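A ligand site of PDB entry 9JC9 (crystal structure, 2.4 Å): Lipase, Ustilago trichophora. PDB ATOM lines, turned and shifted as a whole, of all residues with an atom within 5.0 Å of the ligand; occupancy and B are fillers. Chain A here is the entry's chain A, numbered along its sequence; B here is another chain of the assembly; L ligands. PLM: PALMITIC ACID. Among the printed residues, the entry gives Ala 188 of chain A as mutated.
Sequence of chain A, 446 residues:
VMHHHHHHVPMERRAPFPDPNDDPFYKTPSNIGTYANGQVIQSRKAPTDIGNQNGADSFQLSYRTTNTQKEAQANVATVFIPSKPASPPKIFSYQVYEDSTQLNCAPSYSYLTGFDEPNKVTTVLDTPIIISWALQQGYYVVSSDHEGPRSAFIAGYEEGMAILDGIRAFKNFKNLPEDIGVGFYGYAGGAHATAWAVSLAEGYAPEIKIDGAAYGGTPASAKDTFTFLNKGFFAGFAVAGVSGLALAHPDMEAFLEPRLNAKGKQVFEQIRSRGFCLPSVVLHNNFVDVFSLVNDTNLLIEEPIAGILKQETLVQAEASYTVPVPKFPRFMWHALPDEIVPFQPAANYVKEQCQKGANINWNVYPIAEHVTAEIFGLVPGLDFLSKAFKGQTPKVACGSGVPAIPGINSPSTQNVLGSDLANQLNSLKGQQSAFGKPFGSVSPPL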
ATOM      1  N   TYR A  97      -6.924  11.313  19.041  1.00  0.00           N
ATOM      2  CA  TYR A  97      -7.460  10.702  20.264  1.00  0.00           C
ATOM      3  C   TYR A  97      -8.545  11.620  20.861  1.00  0.00           C
ATOM      4  O   TYR A  97      -8.371  12.275  21.888  1.00  0.00           O
ATOM      5  CB  TYR A  97      -6.332  10.394  21.258  1.00  0.00           C
ATOM      6  CG  TYR A  97      -5.273  11.478  21.356  1.00  0.00           C
ATOM      7  CD1 TYR A  97      -5.443  12.573  22.207  1.00  0.00           C
ATOM      8  CD2 TYR A  97      -4.115  11.432  20.586  1.00  0.00           C
ATOM      9  CE1 TYR A  97      -4.500  13.585  22.284  1.00  0.00           C
ATOM     10  CE2 TYR A  97      -3.169  12.435  20.665  1.00  0.00           C
ATOM     11  CZ  TYR A  97      -3.366  13.510  21.515  1.00  0.00           C
ATOM     12  OH  TYR A  97      -2.422  14.511  21.584  1.00  0.00           O
ATOM     13  N   ASP A  99     -11.477  10.943  22.312  1.00  0.00           N
ATOM     14  CA  ASP A  99     -11.689  10.453  23.683  1.00  0.00           C
ATOM     15  C   ASP A  99     -12.880  11.144  24.359  1.00  0.00           C
ATOM     16  O   ASP A  99     -12.843  11.415  25.566  1.00  0.00           O
ATOM     17  CB  ASP A  99     -10.421  10.618  24.521  1.00  0.00           C
ATOM     18  CG  ASP A  99      -9.248   9.722  24.056  1.00  0.00           C
ATOM     19  OD1 ASP A  99      -9.326   9.030  22.991  1.00  0.00           O
ATOM     20  OD2 ASP A  99      -8.214   9.713  24.776  1.00  0.00           O
ATOM     21  N   PHE A 153     -17.160   6.932  20.781  1.00  0.00           N
ATOM     22  CA  PHE A 153     -15.803   6.619  21.238  1.00  0.00           C
ATOM     23  C   PHE A 153     -15.602   5.117  21.494  1.00  0.00           C
ATOM     24  O   PHE A 153     -16.463   4.436  22.077  1.00  0.00           O
ATOM     25  CB  PHE A 153     -15.524   7.442  22.521  1.00  0.00           C
ATOM     26  CG  PHE A 153     -14.240   7.111  23.220  1.00  0.00           C
ATOM     27  CD1 PHE A 153     -13.052   7.028  22.512  1.00  0.00           C
ATOM     28  CD2 PHE A 153     -14.223   6.918  24.593  1.00  0.00           C
ATOM     29  CE1 PHE A 153     -11.865   6.724  23.166  1.00  0.00           C
ATOM     30  CE2 PHE A 153     -13.048   6.620  25.249  1.00  0.00           C
ATOM     31  CZ  PHE A 153     -11.857   6.517  24.534  1.00  0.00           C
ATOM     32  N   ILE A 154     -14.429   4.613  21.048  1.00  0.00           N
ATOM     33  CA  ILE A 154     -13.930   3.230  20.936  1.00  0.00           C
ATOM     34  C   ILE A 154     -14.923   2.204  20.391  1.00  0.00           C
ATOM     35  O   ILE A 154     -14.782   0.996  20.627  1.00  0.00           O
ATOM     36  CB  ILE A 154     -13.325   2.673  22.253  1.00  0.00           C
ATOM     37  CG1 ILE A 154     -14.263   2.854  23.415  1.00  0.00           C
ATOM     38  CG2 ILE A 154     -11.868   3.164  22.522  1.00  0.00           C
ATOM     39  CD1 ILE A 154     -15.042   1.668  23.675  1.00  0.00           C
ATOM     40  N   ALA A 188      -2.920   6.184  21.056  1.00  0.00           N
ATOM     41  CA  ALA A 188      -3.888   6.149  22.161  1.00  0.00           C
ATOM     42  C   ALA A 188      -5.278   5.939  21.560  1.00  0.00           C
ATOM     43  O   ALA A 188      -5.456   4.972  20.792  1.00  0.00           O
ATOM     44  CB  ALA A 188      -3.717   7.400  23.033  1.00  0.00           C
ATOM     45  N   GLY A 189      -6.268   6.774  21.887  1.00  0.00           N
ATOM     46  CA  GLY A 189      -7.563   6.643  21.248  1.00  0.00           C
ATOM     47  C   GLY A 189      -7.475   6.749  19.740  1.00  0.00           C
ATOM     48  O   GLY A 189      -8.269   6.128  19.027  1.00  0.00           O
ATOM     49  N   PRO A 219      -5.507   0.409  22.320  1.00  0.00           N
ATOM     50  CA  PRO A 219      -6.502  -0.398  23.023  1.00  0.00           C
ATOM     51  C   PRO A 219      -6.984  -1.529  22.131  1.00  0.00           C
ATOM     52  O   PRO A 219      -7.832  -1.308  21.262  1.00  0.00           O
ATOM     53  CB  PRO A 219      -7.623   0.615  23.339  1.00  0.00           C
ATOM     54  CG  PRO A 219      -6.991   1.974  23.155  1.00  0.00           C
ATOM     55  CD  PRO A 219      -5.984   1.779  22.063  1.00  0.00           C
ATOM     56  N   ALA A 222     -11.781  -3.835  23.986  1.00  0.00           N
ATOM     57  CA  ALA A 222     -12.624  -2.936  24.757  1.00  0.00           C
ATOM     58  C   ALA A 222     -12.790  -3.459  26.175  1.00  0.00           C
ATOM     59  O   ALA A 222     -12.687  -2.695  27.146  1.00  0.00           O
ATOM     60  CB  ALA A 222     -13.983  -2.764  24.086  1.00  0.00           C
ATOM     61  N   THR A 225      -9.561  -3.190  28.321  1.00  0.00           N
ATOM     62  CA  THR A 225      -9.227  -1.817  28.669  1.00  0.00           C
ATOM     63  C   THR A 225     -10.149  -1.290  29.751  1.00  0.00           C
ATOM     64  O   THR A 225      -9.716  -0.545  30.644  1.00  0.00           O
ATOM     65  CB  THR A 225      -9.256  -0.915  27.437  1.00  0.00           C
ATOM     66  OG1 THR A 225      -8.505  -1.525  26.393  1.00  0.00           O
ATOM     67  CG2 THR A 225      -8.629   0.422  27.751  1.00  0.00           C
ATOM     68  N   PHE A 226     -11.420  -1.697  29.713  1.00  0.00           N
ATOM     69  CA  PHE A 226     -12.342  -1.298  30.777  1.00  0.00           C
ATOM     70  C   PHE A 226     -11.867  -1.820  32.130  1.00  0.00           C
ATOM     71  O   PHE A 226     -11.787  -1.055  33.096  1.00  0.00           O
ATOM     72  CB  PHE A 226     -13.763  -1.792  30.478  1.00  0.00           C
ATOM     73  CG  PHE A 226     -14.675  -1.684  31.657  1.00  0.00           C
ATOM     74  CD1 PHE A 226     -15.331  -0.482  31.937  1.00  0.00           C
ATOM     75  CD2 PHE A 226     -14.843  -2.775  32.524  1.00  0.00           C
ATOM     76  CE1 PHE A 226     -16.177  -0.371  33.048  1.00  0.00           C
ATOM     77  CE2 PHE A 226     -15.674  -2.669  33.642  1.00  0.00           C
ATOM     78  CZ  PHE A 226     -16.335  -1.471  33.903  1.00  0.00           C
ATOM     79  N   LEU A 229      -8.914  -0.081  33.563  1.00  0.00           N
ATOM     80  CA  LEU A 229      -9.129   1.333  33.892  1.00  0.00           C
ATOM     81  C   LEU A 229     -10.057   1.542  35.077  1.00  0.00           C
ATOM     82  O   LEU A 229      -9.899   2.528  35.794  1.00  0.00           O
ATOM     83  CB  LEU A 229      -9.725   2.054  32.688  1.00  0.00           C
ATOM     84  CG  LEU A 229      -8.739   2.457  31.603  1.00  0.00           C
ATOM     85  CD1 LEU A 229      -9.524   2.969  30.401  1.00  0.00           C
ATOM     86  CD2 LEU A 229      -7.810   3.527  32.155  1.00  0.00           C
ATOM     87  N   PHE A 237     -12.144   7.418  31.693  1.00  0.00           N
ATOM     88  CA  PHE A 237     -12.113   6.847  30.348  1.00  0.00           C
ATOM     89  C   PHE A 237     -13.025   5.631  30.249  1.00  0.00           C
ATOM     90  O   PHE A 237     -13.661   5.397  29.215  1.00  0.00           O
ATOM     91  CB  PHE A 237     -10.679   6.459  29.983  1.00  0.00           C
ATOM     92  CG  PHE A 237      -9.835   7.588  29.487  1.00  0.00           C
ATOM     93  CD1 PHE A 237     -10.257   8.381  28.425  1.00  0.00           C
ATOM     94  CD2 PHE A 237      -8.608   7.849  30.066  1.00  0.00           C
ATOM     95  CE1 PHE A 237      -9.468   9.421  27.948  1.00  0.00           C
ATOM     96  CE2 PHE A 237      -7.819   8.900  29.598  1.00  0.00           C
ATOM     97  CZ  PHE A 237      -8.253   9.688  28.529  1.00  0.00           C
ATOM     98  N   ALA A 238     -13.062   4.816  31.314  1.00  0.00           N
ATOM     99  CA  ALA A 238     -13.993   3.693  31.349  1.00  0.00           C
ATOM    100  C   ALA A 238     -15.436   4.174  31.237  1.00  0.00           C
ATOM    101  O   ALA A 238     -16.239   3.570  30.513  1.00  0.00           O
ATOM    102  CB  ALA A 238     -13.788   2.875  32.637  1.00  0.00           C
ATOM    103  N   GLY A 241     -15.793   5.236  27.605  1.00  0.00           N
ATOM    104  CA  GLY A 241     -15.900   4.109  26.703  1.00  0.00           C
ATOM    105  C   GLY A 241     -17.239   3.399  26.792  1.00  0.00           C
ATOM    106  O   GLY A 241     -17.773   2.914  25.780  1.00  0.00           O
ATOM    107  N   VAL A 242     -17.790   3.310  28.003  1.00  0.00           N
ATOM    108  CA  VAL A 242     -19.132   2.743  28.150  1.00  0.00           C
ATOM    109  C   VAL A 242     -20.131   3.593  27.387  1.00  0.00           C
ATOM    110  O   VAL A 242     -20.986   3.087  26.657  1.00  0.00           O
ATOM    111  CB  VAL A 242     -19.516   2.590  29.635  1.00  0.00           C
ATOM    112  CG1 VAL A 242     -21.015   2.268  29.784  1.00  0.00           C
ATOM    113  CG2 VAL A 242     -18.685   1.505  30.296  1.00  0.00           C
ATOM    114  N   LEU A 245     -19.572   3.023  23.418  1.00  0.00           N
ATOM    115  CA  LEU A 245     -20.141   1.787  22.893  1.00  0.00           C
ATOM    116  C   LEU A 245     -21.665   1.842  22.893  1.00  0.00           C
ATOM    117  O   LEU A 245     -22.307   1.431  21.915  1.00  0.00           O
ATOM    118  CB  LEU A 245     -19.636   0.591  23.696  1.00  0.00           C
ATOM    119  CG  LEU A 245     -18.153   0.285  23.461  1.00  0.00           C
ATOM    120  CD1 LEU A 245     -17.704  -0.920  24.249  1.00  0.00           C
ATOM    121  CD2 LEU A 245     -17.890   0.063  22.003  1.00  0.00           C
ATOM    122  N   MET A 252     -27.480  -2.001  23.667  1.00  0.00           N
ATOM    123  CA  MET A 252     -26.796  -1.799  24.937  1.00  0.00           C
ATOM    124  C   MET A 252     -27.237  -0.496  25.595  1.00  0.00           C
ATOM    125  O   MET A 252     -27.360  -0.433  26.828  1.00  0.00           O
ATOM    126  CB  MET A 252     -25.270  -1.867  24.719  1.00  0.00           C
ATOM    127  CG  MET A 252     -24.392  -1.023  25.672  1.00  0.00           C
ATOM    128  SD  MET A 252     -22.610  -1.212  25.319  1.00  0.00           S
ATOM    129  CE  MET A 252     -21.882  -0.884  26.931  1.00  0.00           C
ATOM    130  N   VAL A 290     -17.649   1.901  37.611  1.00  0.00           N
ATOM    131  CA  VAL A 290     -18.790   1.998  36.659  1.00  0.00           C
ATOM    132  C   VAL A 290     -19.944   1.181  37.257  1.00  0.00           C
ATOM    133  O   VAL A 290     -21.092   1.609  37.135  1.00  0.00           O
ATOM    134  CB  VAL A 290     -18.387   1.561  35.239  1.00  0.00           C
ATOM    135  CG1 VAL A 290     -19.580   1.441  34.300  1.00  0.00           C
ATOM    136  CG2 VAL A 290     -17.344   2.501  34.646  1.00  0.00           C
ATOM    137  N   PHE A 291     -19.618   0.080  37.919  1.00  0.00           N
ATOM    138  CA  PHE A 291     -20.635  -0.818  38.530  1.00  0.00           C
ATOM    139  C   PHE A 291     -21.414  -0.025  39.588  1.00  0.00           C
ATOM    140  O   PHE A 291     -22.603  -0.288  39.744  1.00  0.00           O
ATOM    141  CB  PHE A 291     -19.914  -2.085  39.011  1.00  0.00           C
ATOM    142  CG  PHE A 291     -19.512  -2.989  37.857  1.00  0.00           C
ATOM    143  CD1 PHE A 291     -20.480  -3.542  37.028  1.00  0.00           C
ATOM    144  CD2 PHE A 291     -18.173  -3.270  37.600  1.00  0.00           C
ATOM    145  CE1 PHE A 291     -20.124  -4.366  35.976  1.00  0.00           C
ATOM    146  CE2 PHE A 291     -17.823  -4.086  36.537  1.00  0.00           C
ATOM    147  CZ  PHE A 291     -18.793  -4.637  35.740  1.00  0.00           C
ATOM    148  N   LEU A 299     -23.316  -6.781  34.395  1.00  0.00           N
ATOM    149  CA  LEU A 299     -23.510  -6.287  33.009  1.00  0.00           C
ATOM    150  C   LEU A 299     -22.513  -6.946  32.050  1.00  0.00           C
ATOM    151  O   LEU A 299     -22.942  -7.302  30.935  1.00  0.00           O
ATOM    152  CB  LEU A 299     -23.266  -4.781  33.009  1.00  0.00           C
ATOM    153  CG  LEU A 299     -24.215  -3.930  33.847  1.00  0.00           C
ATOM    154  CD1 LEU A 299     -23.770  -2.491  33.694  1.00  0.00           C
ATOM    155  CD2 LEU A 299     -25.619  -4.095  33.314  1.00  0.00           C
ATOM    156  N   LEU A 300     -21.250  -7.116  32.440  1.00  0.00           N
ATOM    157  CA  LEU A 300     -20.283  -7.680  31.470  1.00  0.00           C
ATOM    158  C   LEU A 300     -20.752  -9.099  31.100  1.00  0.00           C
ATOM    159  O   LEU A 300     -20.641  -9.447  29.913  1.00  0.00           O
ATOM    160  CB  LEU A 300     -18.895  -7.712  32.085  1.00  0.00           C
ATOM    161  CG  LEU A 300     -18.286  -6.371  32.487  1.00  0.00           C
ATOM    162  CD1 LEU A 300     -17.035  -6.604  33.311  1.00  0.00           C
ATOM    163  CD2 LEU A 300     -17.938  -5.580  31.245  1.00  0.00           C
ATOM    164  N   ILE A 305     -24.419  -6.958  26.280  1.00  0.00           N
ATOM    165  CA  ILE A 305     -23.076  -6.390  26.427  1.00  0.00           C
ATOM    166  C   ILE A 305     -22.002  -7.455  26.259  1.00  0.00           C
ATOM    167  O   ILE A 305     -20.985  -7.239  25.599  1.00  0.00           O
ATOM    168  CB  ILE A 305     -22.954  -5.644  27.764  1.00  0.00           C
ATOM    169  CG1 ILE A 305     -23.764  -4.343  27.665  1.00  0.00           C
ATOM    170  CG2 ILE A 305     -21.496  -5.376  28.106  1.00  0.00           C
ATOM    171  CD1 ILE A 305     -23.991  -3.680  28.988  1.00  0.00           C
ATOM    172  N   LEU A 309     -19.060  -6.954  23.561  1.00  0.00           N
ATOM    173  CA  LEU A 309     -17.648  -6.944  23.901  1.00  0.00           C
ATOM    174  C   LEU A 309     -16.865  -7.972  23.095  1.00  0.00           C
ATOM    175  O   LEU A 309     -15.710  -7.732  22.733  1.00  0.00           O
ATOM    176  CB  LEU A 309     -17.485  -7.171  25.401  1.00  0.00           C
ATOM    177  CG  LEU A 309     -17.934  -5.957  26.235  1.00  0.00           C
ATOM    178  CD1 LEU A 309     -17.815  -6.231  27.724  1.00  0.00           C
ATOM    179  CD2 LEU A 309     -17.146  -4.684  25.872  1.00  0.00           C
ATOM    180  N   ILE A 340      -2.585   3.651  31.404  1.00  0.00           N
ATOM    181  CA  ILE A 340      -3.920   3.932  30.885  1.00  0.00           C
ATOM    182  C   ILE A 340      -4.409   2.827  29.959  1.00  0.00           C
ATOM    183  O   ILE A 340      -5.548   2.385  30.073  1.00  0.00           O
ATOM    184  CB  ILE A 340      -3.934   5.307  30.156  1.00  0.00           C
ATOM    185  CG1 ILE A 340      -3.460   6.429  31.083  1.00  0.00           C
ATOM    186  CG2 ILE A 340      -5.329   5.580  29.643  1.00  0.00           C
ATOM    187  CD1 ILE A 340      -3.297   7.759  30.393  1.00  0.00           C
ATOM    188  N   VAL A 341      -3.582   2.389  29.010  1.00  0.00           N
ATOM    189  CA  VAL A 341      -4.021   1.389  28.030  1.00  0.00           C
ATOM    190  C   VAL A 341      -3.157   0.142  28.178  1.00  0.00           C
ATOM    191  O   VAL A 341      -1.947   0.190  27.922  1.00  0.00           O
ATOM    192  CB  VAL A 341      -3.986   1.930  26.588  1.00  0.00           C
ATOM    193  CG1 VAL A 341      -4.312   0.804  25.573  1.00  0.00           C
ATOM    194  CG2 VAL A 341      -4.980   3.094  26.467  1.00  0.00           C
ATOM    195  N   HIS A 370       1.899   5.893  29.314  1.00  0.00           N
ATOM    196  CA  HIS A 370       1.075   6.218  28.158  1.00  0.00           C
ATOM    197  C   HIS A 370       1.507   7.524  27.510  1.00  0.00           C
ATOM    198  O   HIS A 370       1.533   7.641  26.276  1.00  0.00           O
ATOM    199  CB  HIS A 370      -0.388   6.294  28.558  1.00  0.00           C
ATOM    200  CG  HIS A 370      -1.341   6.114  27.424  1.00  0.00           C
ATOM    201  ND1 HIS A 370      -1.496   4.913  26.758  1.00  0.00           N
ATOM    202  CD2 HIS A 370      -2.236   6.968  26.865  1.00  0.00           C
ATOM    203  CE1 HIS A 370      -2.421   5.040  25.831  1.00  0.00           C
ATOM    204  NE2 HIS A 370      -2.889   6.277  25.870  1.00  0.00           N
ATOM    205  N   PHE B 435      -3.591  14.254  28.406  1.00  0.00           N
ATOM    206  CA  PHE B 435      -3.945  13.359  29.491  1.00  0.00           C
ATOM    207  C   PHE B 435      -3.596  13.949  30.853  1.00  0.00           C
ATOM    208  O   PHE B 435      -3.691  13.247  31.869  1.00  0.00           O
ATOM    209  CB  PHE B 435      -3.288  11.995  29.272  1.00  0.00           C
ATOM    210  CG  PHE B 435      -3.636  11.367  27.948  1.00  0.00           C
ATOM    211  CD1 PHE B 435      -2.919  11.716  26.783  1.00  0.00           C
ATOM    212  CD2 PHE B 435      -4.690  10.473  27.834  1.00  0.00           C
ATOM    213  CE1 PHE B 435      -3.258  11.153  25.549  1.00  0.00           C
ATOM    214  CE2 PHE B 435      -5.024   9.903  26.611  1.00  0.00           C
ATOM    215  CZ  PHE B 435      -4.311  10.242  25.459  1.00  0.00           C
HETATM  216  C1  PLM L   1      -6.718   6.714  25.289  1.00  0.00           C
HETATM  217  O1  PLM L   1      -5.739   6.193  25.836  1.00  0.00           O
HETATM  218  O2  PLM L   1      -6.628   7.495  24.332  1.00  0.00           O
HETATM  219  C2  PLM L   1      -8.112   6.393  25.820  1.00  0.00           C
HETATM  220  C3  PLM L   1      -8.195   5.157  26.651  1.00  0.00           C
HETATM  221  C4  PLM L   1      -9.183   4.154  26.112  1.00  0.00           C
HETATM  222  C5  PLM L   1     -10.468   4.067  26.907  1.00  0.00           C
HETATM  223  C6  PLM L   1     -11.387   2.951  26.487  1.00  0.00           C
HETATM  224  C7  PLM L   1     -12.523   2.707  27.443  1.00  0.00           C
HETATM  225  C8  PLM L   1     -12.646   1.278  27.881  1.00  0.00           C
HETATM  226  C9  PLM L   1     -13.698   0.494  27.127  1.00  0.00           C
HETATM  227  CA  PLM L   1     -15.051   0.497  27.786  1.00  0.00           C
HETATM  228  CB  PLM L   1     -15.917  -0.682  27.407  1.00  0.00           C
HETATM  229  CC  PLM L   1     -16.827  -1.154  28.497  1.00  0.00           C
HETATM  230  CD  PLM L   1     -18.176  -1.645  28.012  1.00  0.00           C
HETATM  231  CE  PLM L   1     -18.964  -2.400  29.052  1.00  0.00           C
HETATM  232  CF  PLM L   1     -18.536  -2.138  30.468  1.00  0.00           C
HETATM  233  CG  PLM L   1     -19.663  -2.257  31.471  1.00  0.00           C
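An oxygen (O2) of the ligand lies within hydrogen-bond range of the backbone NH (N) of Gly 189 (2.6 Å). O2 of the ligand lies close to OD2 of Asp 99. O1 of the ligand sits at hydrogen-bond distance from NE2 of His 370, 2.9 Å away.
Residues that only touch the ligand: Phe 153 (3.7 Å), Ile 154 (3.9 Å), Ala 188 (3.2 Å), Ala 222 (3.3 Å), Thr 225 (3.9 Å), Phe 226 (3.7 Å), Leu 229 (3.8 Å), Phe 237 (3.4 Å), Gly 241 (3.7 Å), Val 242 (3.7 Å), Leu 245 (3.6 Å), Met 252 (3.9 Å), Leu 300 (3.6 Å), Leu 309 (3.9 Å), Ile 340 (3.9 Å), Val 341 (3.3 Å) and Phe 435 of chain B (3.7 Å). 20 residues have an atom within 4 Å of the ligand: Asp 99, Phe 153, Ile 154, Ala 188, Gly 189, Ala 222, Thr 225, Phe 226, Leu 229, Phe 237, Gly 241, Val 242, Leu 245, Met 252, Leu 300, Leu 309, Ile 340, Val 341, His 370 and Phe 435 of chain B.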
